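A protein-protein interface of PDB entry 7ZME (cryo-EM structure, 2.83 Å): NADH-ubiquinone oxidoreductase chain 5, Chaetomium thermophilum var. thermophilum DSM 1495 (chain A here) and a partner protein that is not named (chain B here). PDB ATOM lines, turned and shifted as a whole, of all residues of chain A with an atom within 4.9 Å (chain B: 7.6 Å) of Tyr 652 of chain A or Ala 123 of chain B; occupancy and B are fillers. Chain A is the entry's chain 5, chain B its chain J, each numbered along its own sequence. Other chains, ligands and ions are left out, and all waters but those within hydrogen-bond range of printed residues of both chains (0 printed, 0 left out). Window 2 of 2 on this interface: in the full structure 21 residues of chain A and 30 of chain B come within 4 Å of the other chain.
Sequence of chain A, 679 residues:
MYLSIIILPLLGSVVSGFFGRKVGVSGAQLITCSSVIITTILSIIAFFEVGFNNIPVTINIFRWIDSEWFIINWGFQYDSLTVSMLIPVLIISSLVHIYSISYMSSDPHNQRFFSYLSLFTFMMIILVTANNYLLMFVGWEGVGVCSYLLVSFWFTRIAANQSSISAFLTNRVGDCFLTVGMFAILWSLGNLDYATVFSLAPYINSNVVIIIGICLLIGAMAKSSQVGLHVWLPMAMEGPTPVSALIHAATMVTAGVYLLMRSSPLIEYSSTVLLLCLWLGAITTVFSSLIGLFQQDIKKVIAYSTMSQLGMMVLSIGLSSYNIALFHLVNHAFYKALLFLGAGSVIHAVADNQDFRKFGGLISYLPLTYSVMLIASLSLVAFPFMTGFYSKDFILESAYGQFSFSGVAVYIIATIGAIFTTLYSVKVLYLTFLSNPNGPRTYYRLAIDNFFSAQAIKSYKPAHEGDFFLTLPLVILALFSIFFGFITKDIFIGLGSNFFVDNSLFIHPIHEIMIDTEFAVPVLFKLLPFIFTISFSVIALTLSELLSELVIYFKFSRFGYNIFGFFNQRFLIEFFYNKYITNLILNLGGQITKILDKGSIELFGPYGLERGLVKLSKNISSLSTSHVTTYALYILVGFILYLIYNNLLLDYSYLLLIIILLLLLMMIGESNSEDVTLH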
ATOM      1  N   TYR A 645     -36.333  18.949 -11.696  1.00  0.00           N
ATOM      2  CA  TYR A 645     -35.431  17.885 -11.273  1.00  0.00           C
ATOM      3  C   TYR A 645     -35.658  17.496  -9.821  1.00  0.00           C
ATOM      4  O   TYR A 645     -35.623  16.310  -9.477  1.00  0.00           O
ATOM      5  CB  TYR A 645     -33.981  18.300 -11.486  1.00  0.00           C
ATOM      6  CG  TYR A 645     -33.018  17.178 -11.205  1.00  0.00           C
ATOM      7  CD1 TYR A 645     -33.042  16.012 -11.959  1.00  0.00           C
ATOM      8  CD2 TYR A 645     -32.116  17.259 -10.158  1.00  0.00           C
ATOM      9  CE1 TYR A 645     -32.172  14.975 -11.694  1.00  0.00           C
ATOM     10  CE2 TYR A 645     -31.243  16.232  -9.892  1.00  0.00           C
ATOM     11  CZ  TYR A 645     -31.275  15.093 -10.662  1.00  0.00           C
ATOM     12  OH  TYR A 645     -30.406  14.067 -10.392  1.00  0.00           O
ATOM     13  N   LEU A 650     -36.716  12.948 -10.419  1.00  0.00           N
ATOM     14  CA  LEU A 650     -36.250  12.321 -11.644  1.00  0.00           C
ATOM     15  C   LEU A 650     -34.988  11.503 -11.383  1.00  0.00           C
ATOM     16  O   LEU A 650     -34.272  11.706 -10.398  1.00  0.00           O
ATOM     17  CB  LEU A 650     -35.966  13.376 -12.712  1.00  0.00           C
ATOM     18  CG  LEU A 650     -37.084  14.368 -13.025  1.00  0.00           C
ATOM     19  CD1 LEU A 650     -36.602  15.411 -14.018  1.00  0.00           C
ATOM     20  CD2 LEU A 650     -38.303  13.639 -13.564  1.00  0.00           C
ATOM     21  N   ASP A 651     -34.728  10.559 -12.281  1.00  0.00           N
ATOM     22  CA  ASP A 651     -33.461   9.845 -12.257  1.00  0.00           C
ATOM     23  C   ASP A 651     -32.345  10.764 -12.733  1.00  0.00           C
ATOM     24  O   ASP A 651     -32.544  11.596 -13.622  1.00  0.00           O
ATOM     25  CB  ASP A 651     -33.534   8.599 -13.139  1.00  0.00           C
ATOM     26  CG  ASP A 651     -32.388   7.640 -12.888  1.00  0.00           C
ATOM     27  OD1 ASP A 651     -31.737   7.753 -11.827  1.00  0.00           O
ATOM     28  OD2 ASP A 651     -32.137   6.773 -13.751  1.00  0.00           O
ATOM     29  N   TYR A 652     -31.165  10.622 -12.130  1.00  0.00           N
ATOM     30  CA  TYR A 652     -30.041  11.460 -12.526  1.00  0.00           C
ATOM     31  C   TYR A 652     -29.556  11.142 -13.932  1.00  0.00           C
ATOM     32  O   TYR A 652     -28.888  11.979 -14.546  1.00  0.00           O
ATOM     33  CB  TYR A 652     -28.889  11.317 -11.532  1.00  0.00           C
ATOM     34  CG  TYR A 652     -28.293   9.932 -11.454  1.00  0.00           C
ATOM     35  CD1 TYR A 652     -28.806   8.984 -10.578  1.00  0.00           C
ATOM     36  CD2 TYR A 652     -27.209   9.575 -12.245  1.00  0.00           C
ATOM     37  CE1 TYR A 652     -28.262   7.719 -10.497  1.00  0.00           C
ATOM     38  CE2 TYR A 652     -26.658   8.313 -12.171  1.00  0.00           C
ATOM     39  CZ  TYR A 652     -27.189   7.389 -11.294  1.00  0.00           C
ATOM     40  OH  TYR A 652     -26.645   6.128 -11.213  1.00  0.00           O
ATOM     41  N   SER A 653     -29.872   9.955 -14.449  1.00  0.00           N
ATOM     42  CA  SER A 653     -29.532   9.640 -15.831  1.00  0.00           C
ATOM     43  C   SER A 653     -30.246  10.578 -16.793  1.00  0.00           C
ATOM     44  O   SER A 653     -29.667  11.012 -17.795  1.00  0.00           O
ATOM     45  CB  SER A 653     -29.890   8.188 -16.138  1.00  0.00           C
ATOM     46  OG  SER A 653     -31.294   8.024 -16.167  1.00  0.00           O
ATOM     47  N   TYR A 654     -31.512  10.889 -16.506  1.00  0.00           N
ATOM     48  CA  TYR A 654     -32.246  11.851 -17.317  1.00  0.00           C
ATOM     49  C   TYR A 654     -31.524  13.188 -17.366  1.00  0.00           C
ATOM     50  O   TYR A 654     -31.353  13.774 -18.439  1.00  0.00           O
ATOM     51  CB  TYR A 654     -33.659  12.025 -16.765  1.00  0.00           C
ATOM     52  CG  TYR A 654     -34.516  10.789 -16.872  1.00  0.00           C
ATOM     53  CD1 TYR A 654     -34.603  10.083 -18.065  1.00  0.00           C
ATOM     54  CD2 TYR A 654     -35.249  10.333 -15.788  1.00  0.00           C
ATOM     55  CE1 TYR A 654     -35.388   8.953 -18.172  1.00  0.00           C
ATOM     56  CE2 TYR A 654     -36.038   9.202 -15.885  1.00  0.00           C
ATOM     57  CZ  TYR A 654     -36.104   8.517 -17.080  1.00  0.00           C
ATOM     58  OH  TYR A 654     -36.889   7.392 -17.180  1.00  0.00           O
ATOM     59  N   LEU A 655     -31.079  13.681 -16.208  1.00  0.00           N
ATOM     60  CA  LEU A 655     -30.366  14.953 -16.174  1.00  0.00           C
ATOM     61  C   LEU A 655     -29.076  14.892 -16.979  1.00  0.00           C
ATOM     62  O   LEU A 655     -28.771  15.816 -17.740  1.00  0.00           O
ATOM     63  CB  LEU A 655     -30.100  15.361 -14.724  1.00  0.00           C
ATOM     64  CG  LEU A 655     -29.617  16.793 -14.503  1.00  0.00           C
ATOM     65  CD1 LEU A 655     -30.215  17.370 -13.257  1.00  0.00           C
ATOM     66  CD2 LEU A 655     -28.114  16.776 -14.352  1.00  0.00           C
ATOM     67  N   LEU A 656     -28.307  13.814 -16.833  1.00  0.00           N
ATOM     68  CA  LEU A 656     -27.129  13.645 -17.677  1.00  0.00           C
ATOM     69  C   LEU A 656     -27.519  13.512 -19.141  1.00  0.00           C
ATOM     70  O   LEU A 656     -26.842  14.053 -20.023  1.00  0.00           O
ATOM     71  CB  LEU A 656     -26.324  12.431 -17.227  1.00  0.00           C
ATOM     72  CG  LEU A 656     -25.335  12.686 -16.098  1.00  0.00           C
ATOM     73  CD1 LEU A 656     -24.656  11.395 -15.715  1.00  0.00           C
ATOM     74  CD2 LEU A 656     -24.311  13.728 -16.509  1.00  0.00           C
ATOM     75  N   TYR B  69     -33.868   5.833 -24.892  1.00  0.00           N
ATOM     76  CA  TYR B  69     -33.027   5.509 -23.747  1.00  0.00           C
ATOM     77  C   TYR B  69     -33.746   4.595 -22.768  1.00  0.00           C
ATOM     78  O   TYR B  69     -33.167   3.616 -22.291  1.00  0.00           O
ATOM     79  CB  TYR B  69     -32.570   6.776 -23.029  1.00  0.00           C
ATOM     80  CG  TYR B  69     -31.846   6.484 -21.735  1.00  0.00           C
ATOM     81  CD1 TYR B  69     -30.789   5.588 -21.697  1.00  0.00           C
ATOM     82  CD2 TYR B  69     -32.229   7.087 -20.547  1.00  0.00           C
ATOM     83  CE1 TYR B  69     -30.131   5.307 -20.522  1.00  0.00           C
ATOM     84  CE2 TYR B  69     -31.573   6.811 -19.365  1.00  0.00           C
ATOM     85  CZ  TYR B  69     -30.525   5.921 -19.362  1.00  0.00           C
ATOM     86  OH  TYR B  69     -29.868   5.645 -18.190  1.00  0.00           O
ATOM     87  N   TRP B  85     -24.578  -1.373 -13.806  1.00  0.00           N
ATOM     88  CA  TRP B  85     -24.166  -0.198 -14.565  1.00  0.00           C
ATOM     89  C   TRP B  85     -24.326  -0.398 -16.065  1.00  0.00           C
ATOM     90  O   TRP B  85     -24.524   0.575 -16.799  1.00  0.00           O
ATOM     91  CB  TRP B  85     -22.713   0.149 -14.246  1.00  0.00           C
ATOM     92  CG  TRP B  85     -21.744  -0.858 -14.780  1.00  0.00           C
ATOM     93  CD1 TRP B  85     -21.363  -2.023 -14.185  1.00  0.00           C
ATOM     94  CD2 TRP B  85     -21.048  -0.801 -16.029  1.00  0.00           C
ATOM     95  NE1 TRP B  85     -20.466  -2.691 -14.981  1.00  0.00           N
ATOM     96  CE2 TRP B  85     -20.258  -1.962 -16.121  1.00  0.00           C
ATOM     97  CE3 TRP B  85     -21.016   0.120 -17.079  1.00  0.00           C
ATOM     98  CZ2 TRP B  85     -19.442  -2.226 -17.217  1.00  0.00           C
ATOM     99  CZ3 TRP B  85     -20.206  -0.144 -18.168  1.00  0.00           C
ATOM    100  CH2 TRP B  85     -19.430  -1.307 -18.228  1.00  0.00           C
ATOM    101  N   ASN B  88     -27.430   0.886 -18.351  1.00  0.00           N
ATOM    102  CA  ASN B  88     -27.435   2.277 -18.782  1.00  0.00           C
ATOM    103  C   ASN B  88     -26.444   2.531 -19.907  1.00  0.00           C
ATOM    104  O   ASN B  88     -26.546   3.559 -20.583  1.00  0.00           O
ATOM    105  CB  ASN B  88     -27.125   3.193 -17.601  1.00  0.00           C
ATOM    106  CG  ASN B  88     -28.249   3.243 -16.597  1.00  0.00           C
ATOM    107  OD1 ASN B  88     -28.913   4.266 -16.445  1.00  0.00           O
ATOM    108  ND2 ASN B  88     -28.472   2.134 -15.901  1.00  0.00           N
ATOM    109  N   GLY B 117     -23.278   6.814 -24.261  1.00  0.00           N
ATOM    110  CA  GLY B 117     -23.170   5.527 -23.599  1.00  0.00           C
ATOM    111  C   GLY B 117     -22.074   5.488 -22.552  1.00  0.00           C
ATOM    112  O   GLY B 117     -22.252   4.906 -21.481  1.00  0.00           O
ATOM    113  N   VAL B 118     -20.926   6.096 -22.851  1.00  0.00           N
ATOM    114  CA  VAL B 118     -19.821   6.104 -21.898  1.00  0.00           C
ATOM    115  C   VAL B 118     -20.139   7.000 -20.710  1.00  0.00           C
ATOM    116  O   VAL B 118     -19.839   6.653 -19.562  1.00  0.00           O
ATOM    117  CB  VAL B 118     -18.513   6.521 -22.594  1.00  0.00           C
ATOM    118  CG1 VAL B 118     -17.390   6.635 -21.582  1.00  0.00           C
ATOM    119  CG2 VAL B 118     -18.142   5.500 -23.651  1.00  0.00           C
ATOM    120  N   VAL B 119     -20.740   8.165 -20.960  1.00  0.00           N
ATOM    121  CA  VAL B 119     -21.093   9.061 -19.862  1.00  0.00           C
ATOM    122  C   VAL B 119     -22.076   8.385 -18.921  1.00  0.00           C
ATOM    123  O   VAL B 119     -21.917   8.414 -17.696  1.00  0.00           O
ATOM    124  CB  VAL B 119     -21.657  10.387 -20.401  1.00  0.00           C
ATOM    125  CG1 VAL B 119     -22.174  11.234 -19.256  1.00  0.00           C
ATOM    126  CG2 VAL B 119     -20.584  11.147 -21.152  1.00  0.00           C
ATOM    127  N   LEU B 120     -23.102   7.754 -19.483  1.00  0.00           N
ATOM    128  CA  LEU B 120     -24.142   7.165 -18.654  1.00  0.00           C
ATOM    129  C   LEU B 120     -23.674   5.882 -17.984  1.00  0.00           C
ATOM    130  O   LEU B 120     -24.122   5.571 -16.877  1.00  0.00           O
ATOM    131  CB  LEU B 120     -25.397   6.924 -19.494  1.00  0.00           C
ATOM    132  CG  LEU B 120     -26.393   8.088 -19.467  1.00  0.00           C
ATOM    133  CD1 LEU B 120     -25.792   9.340 -20.064  1.00  0.00           C
ATOM    134  CD2 LEU B 120     -27.664   7.731 -20.197  1.00  0.00           C
ATOM    135  N   ALA B 121     -22.774   5.135 -18.627  1.00  0.00           N
ATOM    136  CA  ALA B 121     -22.170   3.982 -17.971  1.00  0.00           C
ATOM    137  C   ALA B 121     -21.264   4.411 -16.825  1.00  0.00           C
ATOM    138  O   ALA B 121     -21.243   3.773 -15.766  1.00  0.00           O
ATOM    139  CB  ALA B 121     -21.386   3.151 -18.983  1.00  0.00           C
ATOM    140  N   THR B 122     -20.507   5.490 -17.023  1.00  0.00           N
ATOM    141  CA  THR B 122     -19.551   5.938 -16.018  1.00  0.00           C
ATOM    142  C   THR B 122     -20.247   6.407 -14.749  1.00  0.00           C
ATOM    143  O   THR B 122     -19.721   6.215 -13.648  1.00  0.00           O
ATOM    144  CB  THR B 122     -18.686   7.056 -16.593  1.00  0.00           C
ATOM    145  OG1 THR B 122     -18.040   6.587 -17.781  1.00  0.00           O
ATOM    146  CG2 THR B 122     -17.626   7.483 -15.595  1.00  0.00           C
ATOM    147  N   ALA B 123     -21.427   7.009 -14.877  1.00  0.00           N
ATOM    148  CA  ALA B 123     -22.152   7.500 -13.714  1.00  0.00           C
ATOM    149  C   ALA B 123     -22.906   6.407 -12.971  1.00  0.00           C
ATOM    150  O   ALA B 123     -23.360   6.652 -11.849  1.00  0.00           O
ATOM    151  CB  ALA B 123     -23.125   8.600 -14.132  1.00  0.00           C
ATOM    152  N   GLU B 124     -23.060   5.223 -13.557  1.00  0.00           N
ATOM    153  CA  GLU B 124     -23.708   4.130 -12.845  1.00  0.00           C
ATOM    154  C   GLU B 124     -22.706   3.242 -12.124  1.00  0.00           C
ATOM    155  O   GLU B 124     -22.976   2.788 -11.007  1.00  0.00           O
ATOM    156  CB  GLU B 124     -24.541   3.284 -13.805  1.00  0.00           C
ATOM    157  CG  GLU B 124     -25.557   4.070 -14.569  1.00  0.00           C
ATOM    158  CD  GLU B 124     -26.754   4.444 -13.733  1.00  0.00           C
ATOM    159  OE1 GLU B 124     -27.303   3.558 -13.049  1.00  0.00           O
ATOM    160  OE2 GLU B 124     -27.145   5.628 -13.763  1.00  0.00           O
ATOM    161  N   TYR B 125     -21.558   2.978 -12.746  1.00  0.00           N
ATOM    162  CA  TYR B 125     -20.507   2.253 -12.045  1.00  0.00           C
ATOM    163  C   TYR B 125     -19.996   3.064 -10.863  1.00  0.00           C
ATOM    164  O   TYR B 125     -19.784   2.524  -9.771  1.00  0.00           O
ATOM    165  CB  TYR B 125     -19.367   1.922 -13.007  1.00  0.00           C
ATOM    166  CG  TYR B 125     -18.454   0.825 -12.512  1.00  0.00           C
ATOM    167  CD1 TYR B 125     -17.541   1.056 -11.491  1.00  0.00           C
ATOM    168  CD2 TYR B 125     -18.505  -0.444 -13.068  1.00  0.00           C
ATOM    169  CE1 TYR B 125     -16.709   0.054 -11.037  1.00  0.00           C
ATOM    170  CE2 TYR B 125     -17.677  -1.453 -12.622  1.00  0.00           C
ATOM    171  CZ  TYR B 125     -16.780  -1.200 -11.606  1.00  0.00           C
ATOM    172  OH  TYR B 125     -15.952  -2.204 -11.160  1.00  0.00           O
ATOM    173  N   ALA B 126     -19.800   4.366 -11.061  1.00  0.00           N
ATOM    174  CA  ALA B 126     -19.386   5.239  -9.975  1.00  0.00           C
ATOM    175  C   ALA B 126     -20.531   5.583  -9.035  1.00  0.00           C
ATOM    176  O   ALA B 126     -20.284   5.884  -7.863  1.00  0.00           O
ATOM    177  CB  ALA B 126     -18.774   6.525 -10.534  1.00  0.00           C
ATOM    178  N   GLY B 127     -21.771   5.541  -9.517  1.00  0.00           N
ATOM    179  CA  GLY B 127     -22.893   5.982  -8.717  1.00  0.00           C
ATOM    180  C   GLY B 127     -22.804   7.467  -8.445  1.00  0.00           C
ATOM    181  O   GLY B 127     -22.572   7.880  -7.306  1.00  0.00           O
ATOM    182  N   SER B 128     -22.966   8.274  -9.495  1.00  0.00           N
ATOM    183  CA  SER B 128     -22.762   9.713  -9.384  1.00  0.00           C
ATOM    184  C   SER B 128     -23.654  10.301  -8.300  1.00  0.00           C
ATOM    185  O   SER B 128     -24.856  10.029  -8.250  1.00  0.00           O
ATOM    186  CB  SER B 128     -23.038  10.390 -10.726  1.00  0.00           C
ATOM    187  OG  SER B 128     -24.422  10.380 -11.026  1.00  0.00           O
ATOM    188  N   GLY B 129     -23.057  11.118  -7.438  1.00  0.00           N
ATOM    189  CA  GLY B 129     -23.745  11.628  -6.270  1.00  0.00           C
ATOM    190  C   GLY B 129     -24.693  12.773  -6.548  1.00  0.00           C
ATOM    191  O   GLY B 129     -24.970  13.574  -5.651  1.00  0.00           O
ATOM    192  N   LEU B 130     -25.205  12.859  -7.779  1.00  0.00           N
ATOM    193  CA  LEU B 130     -26.125  13.938  -8.126  1.00  0.00           C
ATOM    194  C   LEU B 130     -27.377  13.890  -7.262  1.00  0.00           C
ATOM    195  O   LEU B 130     -27.855  14.927  -6.786  1.00  0.00           O
ATOM    196  CB  LEU B 130     -26.495  13.863  -9.609  1.00  0.00           C
ATOM    197  CG  LEU B 130     -25.547  14.491 -10.639  1.00  0.00           C
ATOM    198  CD1 LEU B 130     -25.416  15.993 -10.424  1.00  0.00           C
ATOM    199  CD2 LEU B 130     -24.181  13.823 -10.645  1.00  0.00           C
ATOM    200  N   ARG B 131     -27.925  12.695  -7.047  1.00  0.00           N
ATOM    201  CA  ARG B 131     -29.037  12.493  -6.131  1.00  0.00           C
ATOM    202  C   ARG B 131     -28.570  12.071  -4.742  1.00  0.00           C
ATOM    203  O   ARG B 131     -29.401  11.858  -3.855  1.00  0.00           O
ATOM    204  CB  ARG B 131     -30.006  11.450  -6.712  1.00  0.00           C
ATOM    205  CG  ARG B 131     -31.382  11.408  -6.059  1.00  0.00           C
ATOM    206  CD  ARG B 131     -32.129  12.719  -6.238  1.00  0.00           C
ATOM    207  NE  ARG B 131     -32.830  12.788  -7.516  1.00  0.00           N
ATOM    208  CZ  ARG B 131     -33.409  13.886  -7.990  1.00  0.00           C
ATOM    209  NH1 ARG B 131     -34.028  13.859  -9.161  1.00  0.00           N
ATOM    210  NH2 ARG B 131     -33.366  15.012  -7.292  1.00  0.00           N
ATOM    211  N   GLY B 132     -27.250  11.975  -4.548  1.00  0.00           N
ATOM    212  CA  GLY B 132     -26.689  11.676  -3.212  1.00  0.00           C
ATOM    213  C   GLY B 132     -25.881  10.392  -3.186  1.00  0.00           C
ATOM    214  O   GLY B 132     -26.375   9.375  -3.710  1.00  0.00           O
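O of Ala 123 of chain B sits at hydrogen-bond distance from OH of Tyr 652 of chain A, 3.4 Å away.
The side-chain hydroxyl of Tyr 69 of chain B sits close to the side-chain hydroxyl of Ser 653 of chain A, at 3.4 Å.
The guanidinium group of Arg 131 of chain B sits at hydrogen-bond distance from the backbone carbonyl oxygen of Leu 650 of chain A (2.5 Å).
The guanidinium group (NH1) of Arg 131 of chain B sits at hydrogen-bond distance from the backbone carbonyl oxygen (O) of Tyr 645 of chain A, 2.9 Å away.
OE2 of Glu 124 of chain B lies within hydrogen-bond range of OH of Tyr 652 of chain A.
Printed residues of chain B within 4 Å of Tyr 645 of chain A: Leu 130 and Arg 131.
Of the printed residues of chain B, Leu 650 of chain A touches Arg 131.
Ala 123 of chain B touches just these residues of chain A: Tyr 652 and Leu 656.
Of the printed residues of chain A, Glu 124 of chain B touches Tyr 652.
Of the printed residues of chain A, Ser 128 of chain B touches Tyr 652 (3.1 Å).
The nearest printed residue of chain A that does not touch Leu 130 of chain B is Leu 655 of chain A (4.8 Å).
The side-chain hydroxyl (OH) of Tyr 69 of chain B lies within hydrogen-bond range of the side-chain amide oxygen (OD1) of Asn 88 of chain B, at 2.4 Å.
The backbone carbonyl oxygen of Ala 123 of chain B sits at hydrogen-bond distance from the backbone NH of Ser 128 of chain B, at 2.9 Å.
The side-chain hydroxyl of Ser 653 of chain A is in hydrogen-bond range of the side-chain carboxylate of Asp 651 of chain A (2.8 Å).
The side-chain carboxylate (OE1) of Glu 124 of chain B is in hydrogen-bond range of the side-chain amide nitrogen (ND2) of Asn 88 of chain B, at 3.4 Å.
Hydrophobic or aromatic side chains of chain A within 4 Å of the printed part of chain B: Tyr 645, Tyr 652 and Leu 656.
Of the 19 printed residues of chain B, 6 touch a printed residue of chain A.
Hydrophobic or aromatic side chains of chain B that line the printed part of chain A: Tyr 69, Ala 123 and Leu 130.
Along chain B the printed residues that touch a printed residue of chain A span positions 69 to 131.
Among the printed residues, no Asp or Glu carboxylate lies within 4 Å of a Lys or Arg side-chain nitrogen of the other chain.
Among the printed residues, pairs that only touch across the chains: Tyr 652 of chain A with Ser 128 of chain B, Leu 656 of chain A with Ala 123 of chain B, Tyr 652 of chain A with Leu 130 of chain B and Tyr 645 of chain A with Leu 130 of chain B.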
